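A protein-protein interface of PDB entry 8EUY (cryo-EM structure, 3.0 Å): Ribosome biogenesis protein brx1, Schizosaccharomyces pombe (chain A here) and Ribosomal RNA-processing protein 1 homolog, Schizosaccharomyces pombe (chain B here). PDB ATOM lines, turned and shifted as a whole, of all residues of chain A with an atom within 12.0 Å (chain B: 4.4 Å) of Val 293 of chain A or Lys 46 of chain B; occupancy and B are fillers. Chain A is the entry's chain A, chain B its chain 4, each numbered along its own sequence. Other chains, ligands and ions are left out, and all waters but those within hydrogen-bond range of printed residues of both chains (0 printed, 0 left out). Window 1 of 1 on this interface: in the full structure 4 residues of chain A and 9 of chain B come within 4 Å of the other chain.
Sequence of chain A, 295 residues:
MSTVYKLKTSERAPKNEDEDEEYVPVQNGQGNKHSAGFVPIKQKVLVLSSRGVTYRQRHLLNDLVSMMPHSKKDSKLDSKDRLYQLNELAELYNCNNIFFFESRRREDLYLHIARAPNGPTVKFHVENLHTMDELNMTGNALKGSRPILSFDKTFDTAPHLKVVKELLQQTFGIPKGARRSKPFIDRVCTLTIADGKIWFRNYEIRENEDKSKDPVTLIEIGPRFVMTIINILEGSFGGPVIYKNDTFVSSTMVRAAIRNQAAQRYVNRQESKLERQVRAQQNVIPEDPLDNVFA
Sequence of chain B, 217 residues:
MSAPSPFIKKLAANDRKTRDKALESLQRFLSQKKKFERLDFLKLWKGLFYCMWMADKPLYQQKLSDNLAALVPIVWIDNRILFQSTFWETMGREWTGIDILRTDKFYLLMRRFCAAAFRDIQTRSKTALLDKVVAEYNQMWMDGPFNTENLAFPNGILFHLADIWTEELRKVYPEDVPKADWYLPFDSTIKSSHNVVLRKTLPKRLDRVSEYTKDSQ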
ATOM      1  N   GLU A 287      10.611  13.309 -40.617  1.00  0.00           N
ATOM      2  CA  GLU A 287      10.349  13.514 -39.201  1.00  0.00           C
ATOM      3  C   GLU A 287      11.652  13.533 -38.411  1.00  0.00           C
ATOM      4  O   GLU A 287      12.555  12.726 -38.646  1.00  0.00           O
ATOM      5  CB  GLU A 287       9.421  12.424 -38.663  1.00  0.00           C
ATOM      6  CG  GLU A 287       9.949  11.004 -38.812  1.00  0.00           C
ATOM      7  CD  GLU A 287       9.685  10.418 -40.186  1.00  0.00           C
ATOM      8  OE1 GLU A 287      10.320  10.874 -41.161  1.00  0.00           O
ATOM      9  OE2 GLU A 287       8.845   9.501 -40.290  1.00  0.00           O
ATOM     10  N   ASP A 288      11.750  14.472 -37.484  1.00  0.00           N
ATOM     11  CA  ASP A 288      12.922  14.550 -36.626  1.00  0.00           C
ATOM     12  C   ASP A 288      12.924  13.367 -35.666  1.00  0.00           C
ATOM     13  O   ASP A 288      11.890  13.068 -35.060  1.00  0.00           O
ATOM     14  CB  ASP A 288      12.925  15.864 -35.849  1.00  0.00           C
ATOM     15  CG  ASP A 288      14.318  16.431 -35.661  1.00  0.00           C
ATOM     16  OD1 ASP A 288      14.990  16.048 -34.681  1.00  0.00           O
ATOM     17  OD2 ASP A 288      14.740  17.261 -36.491  1.00  0.00           O
ATOM     18  N   PRO A 289      14.048  12.666 -35.503  1.00  0.00           N
ATOM     19  CA  PRO A 289      14.085  11.557 -34.537  1.00  0.00           C
ATOM     20  C   PRO A 289      13.958  12.005 -33.092  1.00  0.00           C
ATOM     21  O   PRO A 289      13.873  11.149 -32.203  1.00  0.00           O
ATOM     22  CB  PRO A 289      15.448  10.905 -34.800  1.00  0.00           C
ATOM     23  CG  PRO A 289      16.269  11.978 -35.423  1.00  0.00           C
ATOM     24  CD  PRO A 289      15.323  12.817 -36.225  1.00  0.00           C
ATOM     25  N   LEU A 290      13.938  13.313 -32.829  1.00  0.00           N
ATOM     26  CA  LEU A 290      13.861  13.844 -31.475  1.00  0.00           C
ATOM     27  C   LEU A 290      12.583  14.633 -31.220  1.00  0.00           C
ATOM     28  O   LEU A 290      12.449  15.241 -30.151  1.00  0.00           O
ATOM     29  CB  LEU A 290      15.079  14.728 -31.189  1.00  0.00           C
ATOM     30  CG  LEU A 290      16.450  14.072 -31.341  1.00  0.00           C
ATOM     31  CD1 LEU A 290      17.525  14.965 -30.774  1.00  0.00           C
ATOM     32  CD2 LEU A 290      16.467  12.728 -30.655  1.00  0.00           C
ATOM     33  N   ASP A 291      11.643  14.651 -32.168  1.00  0.00           N
ATOM     34  CA  ASP A 291      10.414  15.408 -31.954  1.00  0.00           C
ATOM     35  C   ASP A 291       9.479  14.704 -30.980  1.00  0.00           C
ATOM     36  O   ASP A 291       8.679  15.361 -30.306  1.00  0.00           O
ATOM     37  CB  ASP A 291       9.705  15.662 -33.287  1.00  0.00           C
ATOM     38  CG  ASP A 291       9.364  14.381 -34.030  1.00  0.00           C
ATOM     39  OD1 ASP A 291       9.566  13.282 -33.472  1.00  0.00           O
ATOM     40  OD2 ASP A 291       8.885  14.474 -35.181  1.00  0.00           O
ATOM     41  N   ASN A 292       9.561  13.378 -30.895  1.00  0.00           N
ATOM     42  CA  ASN A 292       8.708  12.585 -30.021  1.00  0.00           C
ATOM     43  C   ASN A 292       9.499  11.930 -28.893  1.00  0.00           C
ATOM     44  O   ASN A 292       9.159  10.834 -28.443  1.00  0.00           O
ATOM     45  CB  ASN A 292       7.958  11.526 -30.827  1.00  0.00           C
ATOM     46  CG  ASN A 292       8.876  10.721 -31.728  1.00  0.00           C
ATOM     47  OD1 ASN A 292      10.083  10.952 -31.765  1.00  0.00           O
ATOM     48  ND2 ASN A 292       8.306   9.770 -32.457  1.00  0.00           N
ATOM     49  N   VAL A 293      10.566  12.585 -28.437  1.00  0.00           N
ATOM     50  CA  VAL A 293      11.382  12.012 -27.371  1.00  0.00           C
ATOM     51  C   VAL A 293      10.629  12.037 -26.045  1.00  0.00           C
ATOM     52  O   VAL A 293      10.708  11.090 -25.253  1.00  0.00           O
ATOM     53  CB  VAL A 293      12.738  12.739 -27.289  1.00  0.00           C
ATOM     54  CG1 VAL A 293      12.546  14.228 -27.056  1.00  0.00           C
ATOM     55  CG2 VAL A 293      13.607  12.128 -26.214  1.00  0.00           C
ATOM     56  N   PHE A 294       9.884  13.108 -25.783  1.00  0.00           N
ATOM     57  CA  PHE A 294       9.080  13.225 -24.575  1.00  0.00           C
ATOM     58  C   PHE A 294       7.654  12.732 -24.766  1.00  0.00           C
ATOM     59  O   PHE A 294       6.852  12.823 -23.833  1.00  0.00           O
ATOM     60  CB  PHE A 294       9.054  14.677 -24.094  1.00  0.00           C
ATOM     61  CG  PHE A 294      10.411  15.240 -23.801  1.00  0.00           C
ATOM     62  CD1 PHE A 294      11.169  14.747 -22.755  1.00  0.00           C
ATOM     63  CD2 PHE A 294      10.932  16.261 -24.573  1.00  0.00           C
ATOM     64  CE1 PHE A 294      12.416  15.262 -22.486  1.00  0.00           C
ATOM     65  CE2 PHE A 294      12.179  16.778 -24.306  1.00  0.00           C
ATOM     66  CZ  PHE A 294      12.920  16.277 -23.262  1.00  0.00           C
ATOM     67  N   ALA A 295       7.319  12.221 -25.944  1.00  0.00           N
ATOM     68  CA  ALA A 295       5.990  11.690 -26.194  1.00  0.00           C
ATOM     69  C   ALA A 295       5.878  10.267 -25.666  1.00  0.00           C
ATOM     70  O   ALA A 295       4.838   9.624 -25.795  1.00  0.00           O
ATOM     71  CB  ALA A 295       5.670  11.734 -27.673  1.00  0.00           C
ATOM     72  OXT ALA A 295       6.827   9.722 -25.102  1.00  0.00           O
ATOM     73  N   ILE B   8      14.458   9.669 -19.782  1.00  0.00           N
ATOM     74  CA  ILE B   8      14.447  10.959 -20.469  1.00  0.00           C
ATOM     75  C   ILE B   8      13.201  11.766 -20.120  1.00  0.00           C
ATOM     76  O   ILE B   8      13.294  12.951 -19.784  1.00  0.00           O
ATOM     77  CB  ILE B   8      14.571  10.772 -21.991  1.00  0.00           C
ATOM     78  CG1 ILE B   8      15.999  10.371 -22.360  1.00  0.00           C
ATOM     79  CG2 ILE B   8      14.168  12.038 -22.716  1.00  0.00           C
ATOM     80  CD1 ILE B   8      16.210   8.878 -22.451  1.00  0.00           C
ATOM     81  N   LEU B  42      21.913  11.271 -28.061  1.00  0.00           N
ATOM     82  CA  LEU B  42      21.210  12.495 -28.430  1.00  0.00           C
ATOM     83  C   LEU B  42      19.846  12.571 -27.757  1.00  0.00           C
ATOM     84  O   LEU B  42      19.432  13.644 -27.305  1.00  0.00           O
ATOM     85  CB  LEU B  42      21.063  12.580 -29.947  1.00  0.00           C
ATOM     86  CG  LEU B  42      22.305  12.994 -30.734  1.00  0.00           C
ATOM     87  CD1 LEU B  42      22.009  13.003 -32.220  1.00  0.00           C
ATOM     88  CD2 LEU B  42      22.790  14.350 -30.279  1.00  0.00           C
ATOM     89  N   LYS B  43      19.128  11.448 -27.695  1.00  0.00           N
ATOM     90  CA  LYS B  43      17.867  11.417 -26.965  1.00  0.00           C
ATOM     91  C   LYS B  43      18.087  11.652 -25.477  1.00  0.00           C
ATOM     92  O   LYS B  43      17.300  12.349 -24.829  1.00  0.00           O
ATOM     93  CB  LYS B  43      17.155  10.084 -27.186  1.00  0.00           C
ATOM     94  CG  LYS B  43      16.765   9.802 -28.621  1.00  0.00           C
ATOM     95  CD  LYS B  43      16.288   8.371 -28.776  1.00  0.00           C
ATOM     96  CE  LYS B  43      15.660   8.139 -30.136  1.00  0.00           C
ATOM     97  NZ  LYS B  43      14.277   8.679 -30.205  1.00  0.00           N
ATOM     98  N   LEU B  44      19.141  11.060 -24.916  1.00  0.00           N
ATOM     99  CA  LEU B  44      19.439  11.260 -23.503  1.00  0.00           C
ATOM    100  C   LEU B  44      19.772  12.716 -23.210  1.00  0.00           C
ATOM    101  O   LEU B  44      19.312  13.276 -22.209  1.00  0.00           O
ATOM    102  CB  LEU B  44      20.590  10.351 -23.080  1.00  0.00           C
ATOM    103  CG  LEU B  44      21.397  10.798 -21.864  1.00  0.00           C
ATOM    104  CD1 LEU B  44      20.628  10.509 -20.592  1.00  0.00           C
ATOM    105  CD2 LEU B  44      22.751  10.121 -21.842  1.00  0.00           C
ATOM    106  N   TRP B  45      20.565  13.349 -24.073  1.00  0.00           N
ATOM    107  CA  TRP B  45      20.942  14.738 -23.846  1.00  0.00           C
ATOM    108  C   TRP B  45      19.795  15.699 -24.102  1.00  0.00           C
ATOM    109  O   TRP B  45      19.876  16.860 -23.693  1.00  0.00           O
ATOM    110  CB  TRP B  45      22.144  15.106 -24.709  1.00  0.00           C
ATOM    111  CG  TRP B  45      23.420  14.951 -23.971  1.00  0.00           C
ATOM    112  CD1 TRP B  45      24.428  14.088 -24.256  1.00  0.00           C
ATOM    113  CD2 TRP B  45      23.825  15.676 -22.808  1.00  0.00           C
ATOM    114  NE1 TRP B  45      25.441  14.229 -23.344  1.00  0.00           N
ATOM    115  CE2 TRP B  45      25.094  15.200 -22.444  1.00  0.00           C
ATOM    116  CE3 TRP B  45      23.237  16.684 -22.041  1.00  0.00           C
ATOM    117  CZ2 TRP B  45      25.786  15.694 -21.346  1.00  0.00           C
ATOM    118  CZ3 TRP B  45      23.925  17.171 -20.951  1.00  0.00           C
ATOM    119  CH2 TRP B  45      25.185  16.677 -20.613  1.00  0.00           C
ATOM    120  N   LYS B  46      18.739  15.253 -24.778  1.00  0.00           N
ATOM    121  CA  LYS B  46      17.536  16.069 -24.873  1.00  0.00           C
ATOM    122  C   LYS B  46      16.846  16.175 -23.519  1.00  0.00           C
ATOM    123  O   LYS B  46      16.393  17.257 -23.130  1.00  0.00           O
ATOM    124  CB  LYS B  46      16.595  15.483 -25.921  1.00  0.00           C
ATOM    125  CG  LYS B  46      15.351  16.300 -26.171  1.00  0.00           C
ATOM    126  CD  LYS B  46      15.659  17.533 -26.991  1.00  0.00           C
ATOM    127  CE  LYS B  46      14.391  18.154 -27.537  1.00  0.00           C
ATOM    128  NZ  LYS B  46      14.635  19.516 -28.073  1.00  0.00           N
ATOM    129  N   GLY B  47      16.752  15.061 -22.791  1.00  0.00           N
ATOM    130  CA  GLY B  47      16.222  15.110 -21.439  1.00  0.00           C
ATOM    131  C   GLY B  47      17.149  15.808 -20.463  1.00  0.00           C
ATOM    132  O   GLY B  47      16.700  16.567 -19.601  1.00  0.00           O
ATOM    133  N   LEU B  48      18.455  15.556 -20.577  1.00  0.00           N
ATOM    134  CA  LEU B  48      19.414  16.183 -19.674  1.00  0.00           C
ATOM    135  C   LEU B  48      19.515  17.680 -19.909  1.00  0.00           C
ATOM    136  O   LEU B  48      19.814  18.432 -18.976  1.00  0.00           O
ATOM    137  CB  LEU B  48      20.788  15.540 -19.829  1.00  0.00           C
ATOM    138  CG  LEU B  48      21.006  14.199 -19.141  1.00  0.00           C
ATOM    139  CD1 LEU B  48      22.373  13.654 -19.491  1.00  0.00           C
ATOM    140  CD2 LEU B  48      20.854  14.360 -17.648  1.00  0.00           C
ATOM    141  N   PHE B  49      19.296  18.131 -21.145  1.00  0.00           N
ATOM    142  CA  PHE B  49      19.275  19.564 -21.409  1.00  0.00           C
ATOM    143  C   PHE B  49      18.122  20.233 -20.677  1.00  0.00           C
ATOM    144  O   PHE B  49      18.281  21.317 -20.109  1.00  0.00           O
ATOM    145  CB  PHE B  49      19.185  19.818 -22.913  1.00  0.00           C
ATOM    146  CG  PHE B  49      18.679  21.184 -23.270  1.00  0.00           C
ATOM    147  CD1 PHE B  49      19.533  22.269 -23.293  1.00  0.00           C
ATOM    148  CD2 PHE B  49      17.351  21.382 -23.594  1.00  0.00           C
ATOM    149  CE1 PHE B  49      19.068  23.522 -23.621  1.00  0.00           C
ATOM    150  CE2 PHE B  49      16.884  22.631 -23.916  1.00  0.00           C
ATOM    151  CZ  PHE B  49      17.742  23.700 -23.932  1.00  0.00           C
ATOM    152  N   TYR B  50      16.949  19.599 -20.679  1.00  0.00           N
ATOM    153  CA  TYR B  50      15.789  20.161 -20.002  1.00  0.00           C
ATOM    154  C   TYR B  50      15.839  19.974 -18.496  1.00  0.00           C
ATOM    155  O   TYR B  50      15.186  20.730 -17.773  1.00  0.00           O
ATOM    156  CB  TYR B  50      14.509  19.555 -20.571  1.00  0.00           C
ATOM    157  CG  TYR B  50      14.089  20.219 -21.854  1.00  0.00           C
ATOM    158  CD1 TYR B  50      13.558  21.497 -21.849  1.00  0.00           C
ATOM    159  CD2 TYR B  50      14.252  19.582 -23.071  1.00  0.00           C
ATOM    160  CE1 TYR B  50      13.186  22.114 -23.016  1.00  0.00           C
ATOM    161  CE2 TYR B  50      13.881  20.194 -24.245  1.00  0.00           C
ATOM    162  CZ  TYR B  50      13.349  21.460 -24.211  1.00  0.00           C
ATOM    163  OH  TYR B  50      12.977  22.075 -25.381  1.00  0.00           O
ATOM    164  N   ARG B  93      22.611  23.084 -31.279  1.00  0.00           N
ATOM    165  CA  ARG B  93      21.311  23.211 -31.921  1.00  0.00           C
ATOM    166  C   ARG B  93      20.256  23.850 -31.031  1.00  0.00           C
ATOM    167  O   ARG B  93      19.213  24.266 -31.546  1.00  0.00           O
ATOM    168  CB  ARG B  93      20.821  21.842 -32.395  1.00  0.00           C
ATOM    169  CG  ARG B  93      20.241  20.980 -31.304  1.00  0.00           C
ATOM    170  CD  ARG B  93      19.468  19.809 -31.874  1.00  0.00           C
ATOM    171  NE  ARG B  93      19.703  18.594 -31.106  1.00  0.00           N
ATOM    172  CZ  ARG B  93      19.144  18.325 -29.935  1.00  0.00           C
ATOM    173  NH1 ARG B  93      18.294  19.163 -29.367  1.00  0.00           N
ATOM    174  NH2 ARG B  93      19.449  17.189 -29.316  1.00  0.00           N
ATOM    175  N   GLU B  94      20.491  23.950 -29.726  1.00  0.00           N
ATOM    176  CA  GLU B  94      19.532  24.561 -28.819  1.00  0.00           C
ATOM    177  C   GLU B  94      20.007  25.887 -28.249  1.00  0.00           C
ATOM    178  O   GLU B  94      19.268  26.510 -27.487  1.00  0.00           O
ATOM    179  CB  GLU B  94      19.201  23.599 -27.672  1.00  0.00           C
ATOM    180  CG  GLU B  94      18.841  22.201 -28.128  1.00  0.00           C
ATOM    181  CD  GLU B  94      17.497  21.738 -27.606  1.00  0.00           C
ATOM    182  OE1 GLU B  94      16.511  22.490 -27.746  1.00  0.00           O
ATOM    183  OE2 GLU B  94      17.426  20.616 -27.065  1.00  0.00           O
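Leu 290 of chain A touches Lys 43 of chain B.
Arg 93 of chain B touches Leu 290 of chain A.
Val 293 of chain A touches Ile 8 of chain B.
Val 293 of chain A touches Lys 43 of chain B.
Lys 46 of chain B touches Val 293 of chain A.
Phe 294 of chain A touches Ile 8 of chain B.
Phe 294 of chain A touches Lys 46 of chain B.
Phe 294 of chain A touches Gly 47 of chain B.
Phe 294 of chain A touches Tyr 50 of chain B (CZ to CD2, 3.6 Å).
Val 293 of chain A touches just these residues of chain B: Ile 8, Lys 43 and Lys 46.
Lys 46 of chain B touches just these residues of chain A: Val 293 and Phe 294.
Ile 8 of chain B touches just these residues of chain A: Val 293 (3.5 Å) and Phe 294 (3.7 Å).
Lys 43 of chain B touches just these residues of chain A: Pro 289 (3.2 Å), Leu 290 (3.6 Å) and Val 293 (3.95 Å).
No residue of chain A comes within 4 Å of Trp 45 of chain B.
Of chain A, only Phe 294 (3.9 Å) comes within 4 Å of Gly 47 of chain B.
No residue of chain A comes within 4 Å of Leu 48 of chain B.
No residue of chain A comes within 4 Å of Phe 49 of chain B.
Of the printed residues of chain A, Arg 93 of chain B touches Leu 290.
Printed residues of chain B within 4 Å of Phe 294 of chain A: Ile 8, Lys 46, Gly 47 and Tyr 50.
Leu 42 of chain B touches none of the printed residues of chain A.
Asn 292 of chain A touches none of the printed residues of chain B.
The nearest printed residue of chain B that does not touch Val 293 of chain A is Gly 47 of chain B (5.5 Å).
The nearest printed residue of chain B that does not touch Leu 290 of chain A is Leu 42 of chain B (4.2 Å).
Of the 12 printed residues of chain B, 6 touch a printed residue of chain A.
Of the 9 printed residues of chain A, 4 touch a printed residue of chain B.
OE2 of Glu 94 of chain B lies within salt-bridge range of NZ of Lys 46 of chain B, at 3.2 Å.
The guanidinium group (NH1) of Arg 93 of chain B is in salt-bridge range of the side-chain carboxylate (OE2) of Glu 94 of chain B, at 2.9 Å.
OD1 of Asp 288 of chain A lies close to N of Leu 290 of chain A, at 3.5 Å.
The side-chain amino group (NZ) of Lys 43 of chain B lies within hydrogen-bond range of the backbone carbonyl oxygen (O) of Pro 289 of chain A, 3.2 Å away.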
